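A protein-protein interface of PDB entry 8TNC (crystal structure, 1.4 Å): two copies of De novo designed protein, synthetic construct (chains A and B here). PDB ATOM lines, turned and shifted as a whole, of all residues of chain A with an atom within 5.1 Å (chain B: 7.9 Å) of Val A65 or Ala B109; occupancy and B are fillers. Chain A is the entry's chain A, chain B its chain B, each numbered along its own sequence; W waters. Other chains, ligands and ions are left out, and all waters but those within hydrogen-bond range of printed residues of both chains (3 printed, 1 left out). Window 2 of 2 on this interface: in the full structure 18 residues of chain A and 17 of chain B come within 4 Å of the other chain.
Of the 14 printed residues of chain A, 5 touch a printed residue of chain B.
Along chain A the printed residues that touch a printed residue of chain B span positions 62 to 91.
Of the 16 printed residues of chain B, 6 touch a printed residue of chain A.
Printed residues of chain B that touch a printed residue of chain A: Ala B44, Asp B48, Val B105, Ala B106, Ala B109 and Asn B110.
Hydrophobic or aromatic side chains of chain B within 4 Å of the printed part of chain A: Ala B44, Val B105, Ala B106 and Ala B109.
Among the printed residues, Asp or Glu carboxylates within 4 Å of a Lys or Arg side-chain nitrogen of the other chain: Arg A66 with Asp B48 (2.6 Å).
Water W3 bridges OE2 of Glu A88 and O of Asn B110.
Water W1 bridges the guanidinium group (NH2) of Arg A66 (2.8 Å) and the backbone carbonyl oxygen (O) of Val B105 (2.8 Å).
Water W2 bridges the backbone carbonyl oxygen of Glu A88 (2.9 Å) and the side-chain amide oxygen of Asn B110 (3.0 Å).
Among the printed residues, pairs that only touch across the chains: Val A62 with Val B105, Val A65 with Ala B109, Arg A66 with Ala B109 and Leu A91 with Ala B106.
The backbone carbonyl oxygen (O) of Ala B106 sits close to the side-chain amide oxygen (OD1) of Asn B110.
No position is printed for both chains.
Of the 7 pairs that touch across the chains among the printed residues, none has its exchanged pair printed and touching as well.
ND2 of Asn B110 sits close to OE2 of Glu A88 (3.2 Å).
The guanidinium group (NH2) of Arg A66 lies within hydrogen-bond range of the backbone carbonyl oxygen (O) of Ala B44, at 3.4 Å.
The guanidinium group (NH1) of Arg A66 is in salt-bridge range of the side-chain carboxylate (OD2) of Asp B48 (2.6 Å).
Val A65 touches one residue of chain B.
Of chain A, only Val A65 and Arg A66 come within 4 Å of Ala B109.
Printed residues of chain A within 4 Å of Asp B48: Arg A66.
Printed residues of chain A within 4 Å of Ala B106: Leu A91 (3.8 Å).
The nearest residue of chain A that does not touch Ala B109 is Ala A69 (4.2 Å).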
ATOM      1  N   ALA A  61      -6.824  19.478 -19.563  1.00  0.00           N
ATOM      2  CA  ALA A  61      -6.054  20.374 -18.713  1.00  0.00           C
ATOM      3  C   ALA A  61      -4.667  20.649 -19.293  1.00  0.00           C
ATOM      4  O   ALA A  61      -4.138  21.773 -19.194  1.00  0.00           O
ATOM      5  CB  ALA A  61      -5.937  19.796 -17.306  1.00  0.00           C
ATOM      6  N   VAL A  62      -4.064  19.632 -19.905  1.00  0.00           N
ATOM      7  CA  VAL A  62      -2.803  19.814 -20.623  1.00  0.00           C
ATOM      8  C   VAL A  62      -3.000  20.759 -21.800  1.00  0.00           C
ATOM      9  O   VAL A  62      -2.204  21.696 -22.019  1.00  0.00           O
ATOM     10  CB  VAL A  62      -2.257  18.449 -21.078  1.00  0.00           C
ATOM     11  CG1 VAL A  62      -1.050  18.650 -22.039  1.00  0.00           C
ATOM     12  CG2 VAL A  62      -1.835  17.653 -19.882  1.00  0.00           C
ATOM     13  N   GLU A  63      -4.049  20.535 -22.585  1.00  0.00           N
ATOM     14  CA  GLU A  63      -4.314  21.376 -23.752  1.00  0.00           C
ATOM     15  C   GLU A  63      -4.541  22.816 -23.331  1.00  0.00           C
ATOM     16  O   GLU A  63      -4.097  23.761 -24.006  1.00  0.00           O
ATOM     17  CB  GLU A  63      -5.553  20.874 -24.487  1.00  0.00           C
ATOM     18  CG  GLU A  63      -5.336  19.646 -25.321  1.00  0.00           C
ATOM     19  CD  GLU A  63      -6.637  19.051 -25.827  1.00  0.00           C
ATOM     20  OE1 GLU A  63      -7.583  19.820 -26.113  1.00  0.00           O
ATOM     21  OE2 GLU A  63      -6.688  17.815 -26.008  1.00  0.00           O
ATOM     22  N   THR A  64      -5.191  23.019 -22.191  1.00  0.00           N
ATOM     23  CA  THR A  64      -5.464  24.363 -21.685  1.00  0.00           C
ATOM     24  C   THR A  64      -4.159  25.091 -21.344  1.00  0.00           C
ATOM     25  O   THR A  64      -3.974  26.268 -21.702  1.00  0.00           O
ATOM     26  CB  THR A  64      -6.391  24.259 -20.453  1.00  0.00           C
ATOM     27  OG1 THR A  64      -7.660  23.737 -20.859  1.00  0.00           O
ATOM     28  CG2 THR A  64      -6.624  25.620 -19.816  1.00  0.00           C
ATOM     29  N   VAL A  65      -3.241  24.422 -20.652  1.00  0.00           N
ATOM     30  CA  VAL A  65      -1.937  25.000 -20.359  1.00  0.00           C
ATOM     31  C   VAL A  65      -1.188  25.317 -21.646  1.00  0.00           C
ATOM     32  O   VAL A  65      -0.625  26.414 -21.787  1.00  0.00           O
ATOM     33  CB  VAL A  65      -1.136  24.087 -19.422  1.00  0.00           C
ATOM     34  CG1 VAL A  65       0.335  24.530 -19.300  1.00  0.00           C
ATOM     35  CG2 VAL A  65      -1.776  24.057 -18.034  1.00  0.00           C
ATOM     36  N   ARG A  66      -1.194  24.402 -22.616  1.00  0.00           N
ATOM     37  CA  ARG A  66      -0.484  24.670 -23.873  1.00  0.00           C
ATOM     38  C   ARG A  66      -1.056  25.885 -24.593  1.00  0.00           C
ATOM     39  O   ARG A  66      -0.293  26.705 -25.131  1.00  0.00           O
ATOM     40  CB  ARG A  66      -0.563  23.453 -24.787  1.00  0.00           C
ATOM     41  CG  ARG A  66       0.139  22.214 -24.256  1.00  0.00           C
ATOM     42  CD  ARG A  66       0.202  21.193 -25.356  1.00  0.00           C
ATOM     43  NE  ARG A  66       0.778  19.910 -24.961  1.00  0.00           N
ATOM     44  CZ  ARG A  66       0.227  18.736 -25.254  1.00  0.00           C
ATOM     45  NH1 ARG A  66      -0.890  18.658 -25.967  1.00  0.00           N
ATOM     46  NH2 ARG A  66       0.838  17.606 -24.874  1.00  0.00           N
ATOM     47  N   LEU A  67      -2.386  26.013 -24.646  1.00  0.00           N
ATOM     48  CA  LEU A  67      -3.008  27.159 -25.306  1.00  0.00           C
ATOM     49  C   LEU A  67      -2.685  28.460 -24.580  1.00  0.00           C
ATOM     50  O   LEU A  67      -2.439  29.500 -25.223  1.00  0.00           O
ATOM     51  CB  LEU A  67      -4.521  26.949 -25.433  1.00  0.00           C
ATOM     52  CG  LEU A  67      -4.982  25.940 -26.460  1.00  0.00           C
ATOM     53  CD1 LEU A  67      -6.419  25.496 -26.239  1.00  0.00           C
ATOM     54  CD2 LEU A  67      -4.862  26.550 -27.850  1.00  0.00           C
ATOM     55  N   LEU A  68      -2.679  28.451 -23.250  1.00  0.00           N
ATOM     56  CA  LEU A  68      -2.380  29.684 -22.520  1.00  0.00           C
ATOM     57  C   LEU A  68      -0.896  30.028 -22.594  1.00  0.00           C
ATOM     58  O   LEU A  68      -0.535  31.216 -22.588  1.00  0.00           O
ATOM     59  CB  LEU A  68      -2.855  29.582 -21.072  1.00  0.00           C
ATOM     60  CG  LEU A  68      -4.359  29.775 -20.969  1.00  0.00           C
ATOM     61  CD1 LEU A  68      -4.845  29.277 -19.657  1.00  0.00           C
ATOM     62  CD2 LEU A  68      -4.757  31.221 -21.091  1.00  0.00           C
ATOM     63  N   ALA A  69      -0.017  29.029 -22.666  1.00  0.00           N
ATOM     64  CA  ALA A  69       1.385  29.315 -22.949  1.00  0.00           C
ATOM     65  C   ALA A  69       1.543  29.945 -24.329  1.00  0.00           C
ATOM     66  O   ALA A  69       2.360  30.868 -24.502  1.00  0.00           O
ATOM     67  CB  ALA A  69       2.218  28.042 -22.827  1.00  0.00           C
ATOM     68  N   GLU A  70       0.756  29.510 -25.313  1.00  0.00           N
ATOM     69  CA  GLU A  70       0.837  30.108 -26.649  1.00  0.00           C
ATOM     70  C   GLU A  70       0.248  31.516 -26.657  1.00  0.00           C
ATOM     71  O   GLU A  70       0.764  32.415 -27.344  1.00  0.00           O
ATOM     72  CB  GLU A  70       0.132  29.241 -27.685  1.00  0.00           C
ATOM     73  CG  GLU A  70       0.568  29.551 -29.113  1.00  0.00           C
ATOM     74  CD  GLU A  70       2.050  29.233 -29.361  1.00  0.00           C
ATOM     75  OE1 GLU A  70       2.651  29.858 -30.265  1.00  0.00           O
ATOM     76  OE2 GLU A  70       2.615  28.366 -28.647  1.00  0.00           O
ATOM     77  N   LEU A  84      -2.357  31.746 -17.081  1.00  0.00           N
ATOM     78  CA  LEU A  84      -1.481  30.579 -17.201  1.00  0.00           C
ATOM     79  C   LEU A  84      -1.142  30.007 -15.837  1.00  0.00           C
ATOM     80  O   LEU A  84      -1.152  28.781 -15.655  1.00  0.00           O
ATOM     81  CB  LEU A  84      -0.201  30.967 -17.948  1.00  0.00           C
ATOM     82  CG  LEU A  84       0.845  29.868 -18.111  1.00  0.00           C
ATOM     83  CD1 LEU A  84       0.283  28.718 -18.916  1.00  0.00           C
ATOM     84  CD2 LEU A  84       2.127  30.393 -18.792  1.00  0.00           C
ATOM     85  N   ALA A  87      -4.027  28.015 -14.650  1.00  0.00           N
ATOM     86  CA  ALA A  87      -4.174  26.777 -15.419  1.00  0.00           C
ATOM     87  C   ALA A  87      -3.113  25.755 -15.038  1.00  0.00           C
ATOM     88  O   ALA A  87      -3.381  24.544 -15.018  1.00  0.00           O
ATOM     89  CB  ALA A  87      -4.101  27.077 -16.910  1.00  0.00           C
ATOM     90  N   GLU A  88      -1.899  26.216 -14.736  1.00  0.00           N
ATOM     91  CA  GLU A  88      -0.837  25.323 -14.282  1.00  0.00           C
ATOM     92  C   GLU A  88      -1.167  24.719 -12.917  1.00  0.00           C
ATOM     93  O   GLU A  88      -0.925  23.525 -12.686  1.00  0.00           O
ATOM     94  CB  GLU A  88       0.514  26.062 -14.315  1.00  0.00           C
ATOM     95  CG  GLU A  88       0.935  26.368 -15.755  1.00  0.00           C
ATOM     96  CD  GLU A  88       2.210  27.180 -15.907  1.00  0.00           C
ATOM     97  OE1 GLU A  88       2.680  27.743 -14.899  1.00  0.00           O
ATOM     98  OE2 GLU A  88       2.747  27.200 -17.043  1.00  0.00           O
ATOM     99  N   LEU A  91      -3.834  22.127 -13.606  1.00  0.00           N
ATOM    100  CA  LEU A  91      -3.263  20.892 -14.140  1.00  0.00           C
ATOM    101  C   LEU A  91      -2.589  20.078 -13.048  1.00  0.00           C
ATOM    102  O   LEU A  91      -2.736  18.856 -13.003  1.00  0.00           O
ATOM    103  CB  LEU A  91      -2.309  21.209 -15.292  1.00  0.00           C
ATOM    104  CG  LEU A  91      -1.514  20.035 -15.870  1.00  0.00           C
ATOM    105  CD1 LEU A  91      -2.420  18.963 -16.393  1.00  0.00           C
ATOM    106  CD2 LEU A  91      -0.680  20.593 -16.997  1.00  0.00           C
ATOM    107  N   LEU B  43       6.538  17.150 -30.505  1.00  0.00           N
ATOM    108  CA  LEU B  43       6.663  16.539 -29.190  1.00  0.00           C
ATOM    109  C   LEU B  43       5.310  16.484 -28.489  1.00  0.00           C
ATOM    110  O   LEU B  43       4.951  15.450 -27.908  1.00  0.00           O
ATOM    111  CB  LEU B  43       7.697  17.300 -28.359  1.00  0.00           C
ATOM    112  CG  LEU B  43       7.842  16.818 -26.924  1.00  0.00           C
ATOM    113  CD1 LEU B  43       8.272  15.397 -26.864  1.00  0.00           C
ATOM    114  CD2 LEU B  43       8.850  17.759 -26.226  1.00  0.00           C
ATOM    115  N   ALA B  44       4.558  17.584 -28.519  1.00  0.00           N
ATOM    116  CA  ALA B  44       3.266  17.606 -27.835  1.00  0.00           C
ATOM    117  C   ALA B  44       2.336  16.546 -28.396  1.00  0.00           C
ATOM    118  O   ALA B  44       1.624  15.866 -27.642  1.00  0.00           O
ATOM    119  CB  ALA B  44       2.629  18.984 -27.979  1.00  0.00           C
ATOM    120  N   LEU B  47       3.596  13.066 -27.189  1.00  0.00           N
ATOM    121  CA  LEU B  47       3.304  12.915 -25.765  1.00  0.00           C
ATOM    122  C   LEU B  47       1.821  12.652 -25.531  1.00  0.00           C
ATOM    123  O   LEU B  47       1.466  11.807 -24.701  1.00  0.00           O
ATOM    124  CB  LEU B  47       3.759  14.150 -24.993  1.00  0.00           C
ATOM    125  CG  LEU B  47       5.278  14.284 -24.837  1.00  0.00           C
ATOM    126  CD1 LEU B  47       5.587  15.601 -24.148  1.00  0.00           C
ATOM    127  CD2 LEU B  47       5.860  13.080 -24.092  1.00  0.00           C
ATOM    128  N   ASP B  48       0.944  13.334 -26.265  1.00  0.00           N
ATOM    129  CA  ASP B  48      -0.484  13.063 -26.112  1.00  0.00           C
ATOM    130  C   ASP B  48      -0.813  11.638 -26.532  1.00  0.00           C
ATOM    131  O   ASP B  48      -1.581  10.946 -25.841  1.00  0.00           O
ATOM    132  CB  ASP B  48      -1.325  14.073 -26.872  1.00  0.00           C
ATOM    133  CG  ASP B  48      -1.294  15.449 -26.217  1.00  0.00           C
ATOM    134  OD1 ASP B  48      -0.848  15.552 -25.049  1.00  0.00           O
ATOM    135  OD2 ASP B  48      -1.773  16.417 -26.847  1.00  0.00           O
ATOM    136  N   ASP B 102       2.810  11.414 -16.721  1.00  0.00           N
ATOM    137  CA  ASP B 102       1.963  12.597 -16.542  1.00  0.00           C
ATOM    138  C   ASP B 102       2.788  13.811 -16.145  1.00  0.00           C
ATOM    139  O   ASP B 102       2.570  14.920 -16.668  1.00  0.00           O
ATOM    140  CB  ASP B 102       0.889  12.326 -15.487  1.00  0.00           C
ATOM    141  CG  ASP B 102      -0.515  12.204 -16.087  1.00  0.00           C
ATOM    142  OD1 ASP B 102      -1.491  12.460 -15.337  1.00  0.00           O
ATOM    143  OD2 ASP B 102      -0.646  11.880 -17.291  1.00  0.00           O
ATOM    144  N   THR B 103       3.728  13.632 -15.215  1.00  0.00           N
ATOM    145  CA  THR B 103       4.613  14.719 -14.830  1.00  0.00           C
ATOM    146  C   THR B 103       5.402  15.234 -16.027  1.00  0.00           C
ATOM    147  O   THR B 103       5.586  16.450 -16.195  1.00  0.00           O
ATOM    148  CB  THR B 103       5.566  14.224 -13.744  1.00  0.00           C
ATOM    149  OG1 THR B 103       4.798  13.864 -12.586  1.00  0.00           O
ATOM    150  CG2 THR B 103       6.573  15.302 -13.386  1.00  0.00           C
ATOM    151  N   ALA B 104       5.882  14.323 -16.872  1.00  0.00           N
ATOM    152  CA  ALA B 104       6.638  14.755 -18.047  1.00  0.00           C
ATOM    153  C   ALA B 104       5.758  15.566 -19.000  1.00  0.00           C
ATOM    154  O   ALA B 104       6.172  16.618 -19.510  1.00  0.00           O
ATOM    155  CB  ALA B 104       7.244  13.528 -18.728  1.00  0.00           C
ATOM    156  N   VAL B 105       4.528  15.102 -19.236  1.00  0.00           N
ATOM    157  CA  VAL B 105       3.623  15.808 -20.137  1.00  0.00           C
ATOM    158  C   VAL B 105       3.302  17.199 -19.610  1.00  0.00           C
ATOM    159  O   VAL B 105       3.314  18.171 -20.367  1.00  0.00           O
ATOM    160  CB  VAL B 105       2.349  14.987 -20.374  1.00  0.00           C
ATOM    161  CG1 VAL B 105       1.338  15.755 -21.185  1.00  0.00           C
ATOM    162  CG2 VAL B 105       2.658  13.674 -21.067  1.00  0.00           C
ATOM    163  N   ALA B 106       3.059  17.326 -18.299  1.00  0.00           N
ATOM    164  CA  ALA B 106       2.791  18.634 -17.711  1.00  0.00           C
ATOM    165  C   ALA B 106       4.009  19.546 -17.792  1.00  0.00           C
ATOM    166  O   ALA B 106       3.878  20.758 -18.041  1.00  0.00           O
ATOM    167  CB  ALA B 106       2.382  18.461 -16.249  1.00  0.00           C
ATOM    168  N   ALA B 107       5.192  19.007 -17.513  1.00  0.00           N
ATOM    169  CA  ALA B 107       6.400  19.828 -17.589  1.00  0.00           C
ATOM    170  C   ALA B 107       6.619  20.357 -19.004  1.00  0.00           C
ATOM    171  O   ALA B 107       6.949  21.543 -19.192  1.00  0.00           O
ATOM    172  CB  ALA B 107       7.598  19.020 -17.108  1.00  0.00           C
ATOM    173  N   ALA B 108       6.443  19.499 -20.011  1.00  0.00           N
ATOM    174  CA  ALA B 108       6.552  19.960 -21.390  1.00  0.00           C
ATOM    175  C   ALA B 108       5.551  21.064 -21.685  1.00  0.00           C
ATOM    176  O   ALA B 108       5.874  22.060 -22.348  1.00  0.00           O
ATOM    177  CB  ALA B 108       6.383  18.787 -22.342  1.00  0.00           C
ATOM    178  N   ALA B 109       4.328  20.931 -21.180  1.00  0.00           N
ATOM    179  CA  ALA B 109       3.321  21.950 -21.422  1.00  0.00           C
ATOM    180  C   ALA B 109       3.667  23.270 -20.729  1.00  0.00           C
ATOM    181  O   ALA B 109       3.342  24.341 -21.257  1.00  0.00           O
ATOM    182  CB  ALA B 109       1.956  21.429 -20.947  1.00  0.00           C
ATOM    183  N   ASN B 110       4.244  23.201 -19.516  1.00  0.00           N
ATOM    184  CA  ASN B 110       4.664  24.334 -18.698  1.00  0.00           C
ATOM    185  C   ASN B 110       5.955  24.968 -19.218  1.00  0.00           C
ATOM    186  O   ASN B 110       6.380  25.999 -18.685  1.00  0.00           O
ATOM    187  CB  ASN B 110       4.968  23.874 -17.253  1.00  0.00           C
ATOM    188  CG  ASN B 110       3.732  23.831 -16.321  1.00  0.00           C
ATOM    189  OD1 ASN B 110       2.821  22.993 -16.452  1.00  0.00           O
ATOM    190  ND2 ASN B 110       3.730  24.726 -15.341  1.00  0.00           N
ATOM    191  N   GLY B 111       6.621  24.349 -20.187  1.00  0.00           N
ATOM    192  CA  GLY B 111       7.914  24.866 -20.649  1.00  0.00           C
ATOM    193  C   GLY B 111       9.052  24.656 -19.668  1.00  0.00           C
ATOM    194  O   GLY B 111       9.916  25.532 -19.525  1.00  0.00           O
ATOM    195  N   ASP B 112       9.084  23.508 -19.000  1.00  0.00           N
ATOM    196  CA  ASP B 112      10.033  23.198 -17.935  1.00  0.00           C
ATOM    197  C   ASP B 112      10.819  21.964 -18.349  1.00  0.00           C
ATOM    198  O   ASP B 112      10.492  20.828 -17.974  1.00  0.00           O
ATOM    199  CB  ASP B 112       9.271  22.971 -16.637  1.00  0.00           C
ATOM    200  CG  ASP B 112      10.169  22.602 -15.466  1.00  0.00           C
ATOM    201  OD1 ASP B 112      11.398  22.564 -15.630  1.00  0.00           O
ATOM    202  OD2 ASP B 112       9.628  22.317 -14.374  1.00  0.00           O
ATOM    203  N   PHE B 116      10.833  17.909 -17.323  1.00  0.00           N
ATOM    204  CA  PHE B 116      10.474  16.995 -18.400  1.00  0.00           C
ATOM    205  C   PHE B 116      11.515  15.892 -18.580  1.00  0.00           C
ATOM    206  O   PHE B 116      11.176  14.711 -18.632  1.00  0.00           O
ATOM    207  CB  PHE B 116      10.275  17.725 -19.730  1.00  0.00           C
ATOM    208  CG  PHE B 116      10.200  16.781 -20.896  1.00  0.00           C
ATOM    209  CD1 PHE B 116       9.032  16.067 -21.151  1.00  0.00           C
ATOM    210  CD2 PHE B 116      11.304  16.527 -21.690  1.00  0.00           C
ATOM    211  CE1 PHE B 116       8.958  15.172 -22.163  1.00  0.00           C
ATOM    212  CE2 PHE B 116      11.232  15.617 -22.720  1.00  0.00           C
ATOM    213  CZ  PHE B 116      10.060  14.930 -22.959  1.00  0.00           C
HETATM  214  O   HOH W   1       2.833  18.432 -23.148  1.00  0.00           O
HETATM  215  O   HOH W   2       1.134  22.177 -14.124  1.00  0.00           O
HETATM  216  O   HOH W   3       5.210  28.000 -17.400  1.00  0.00           O
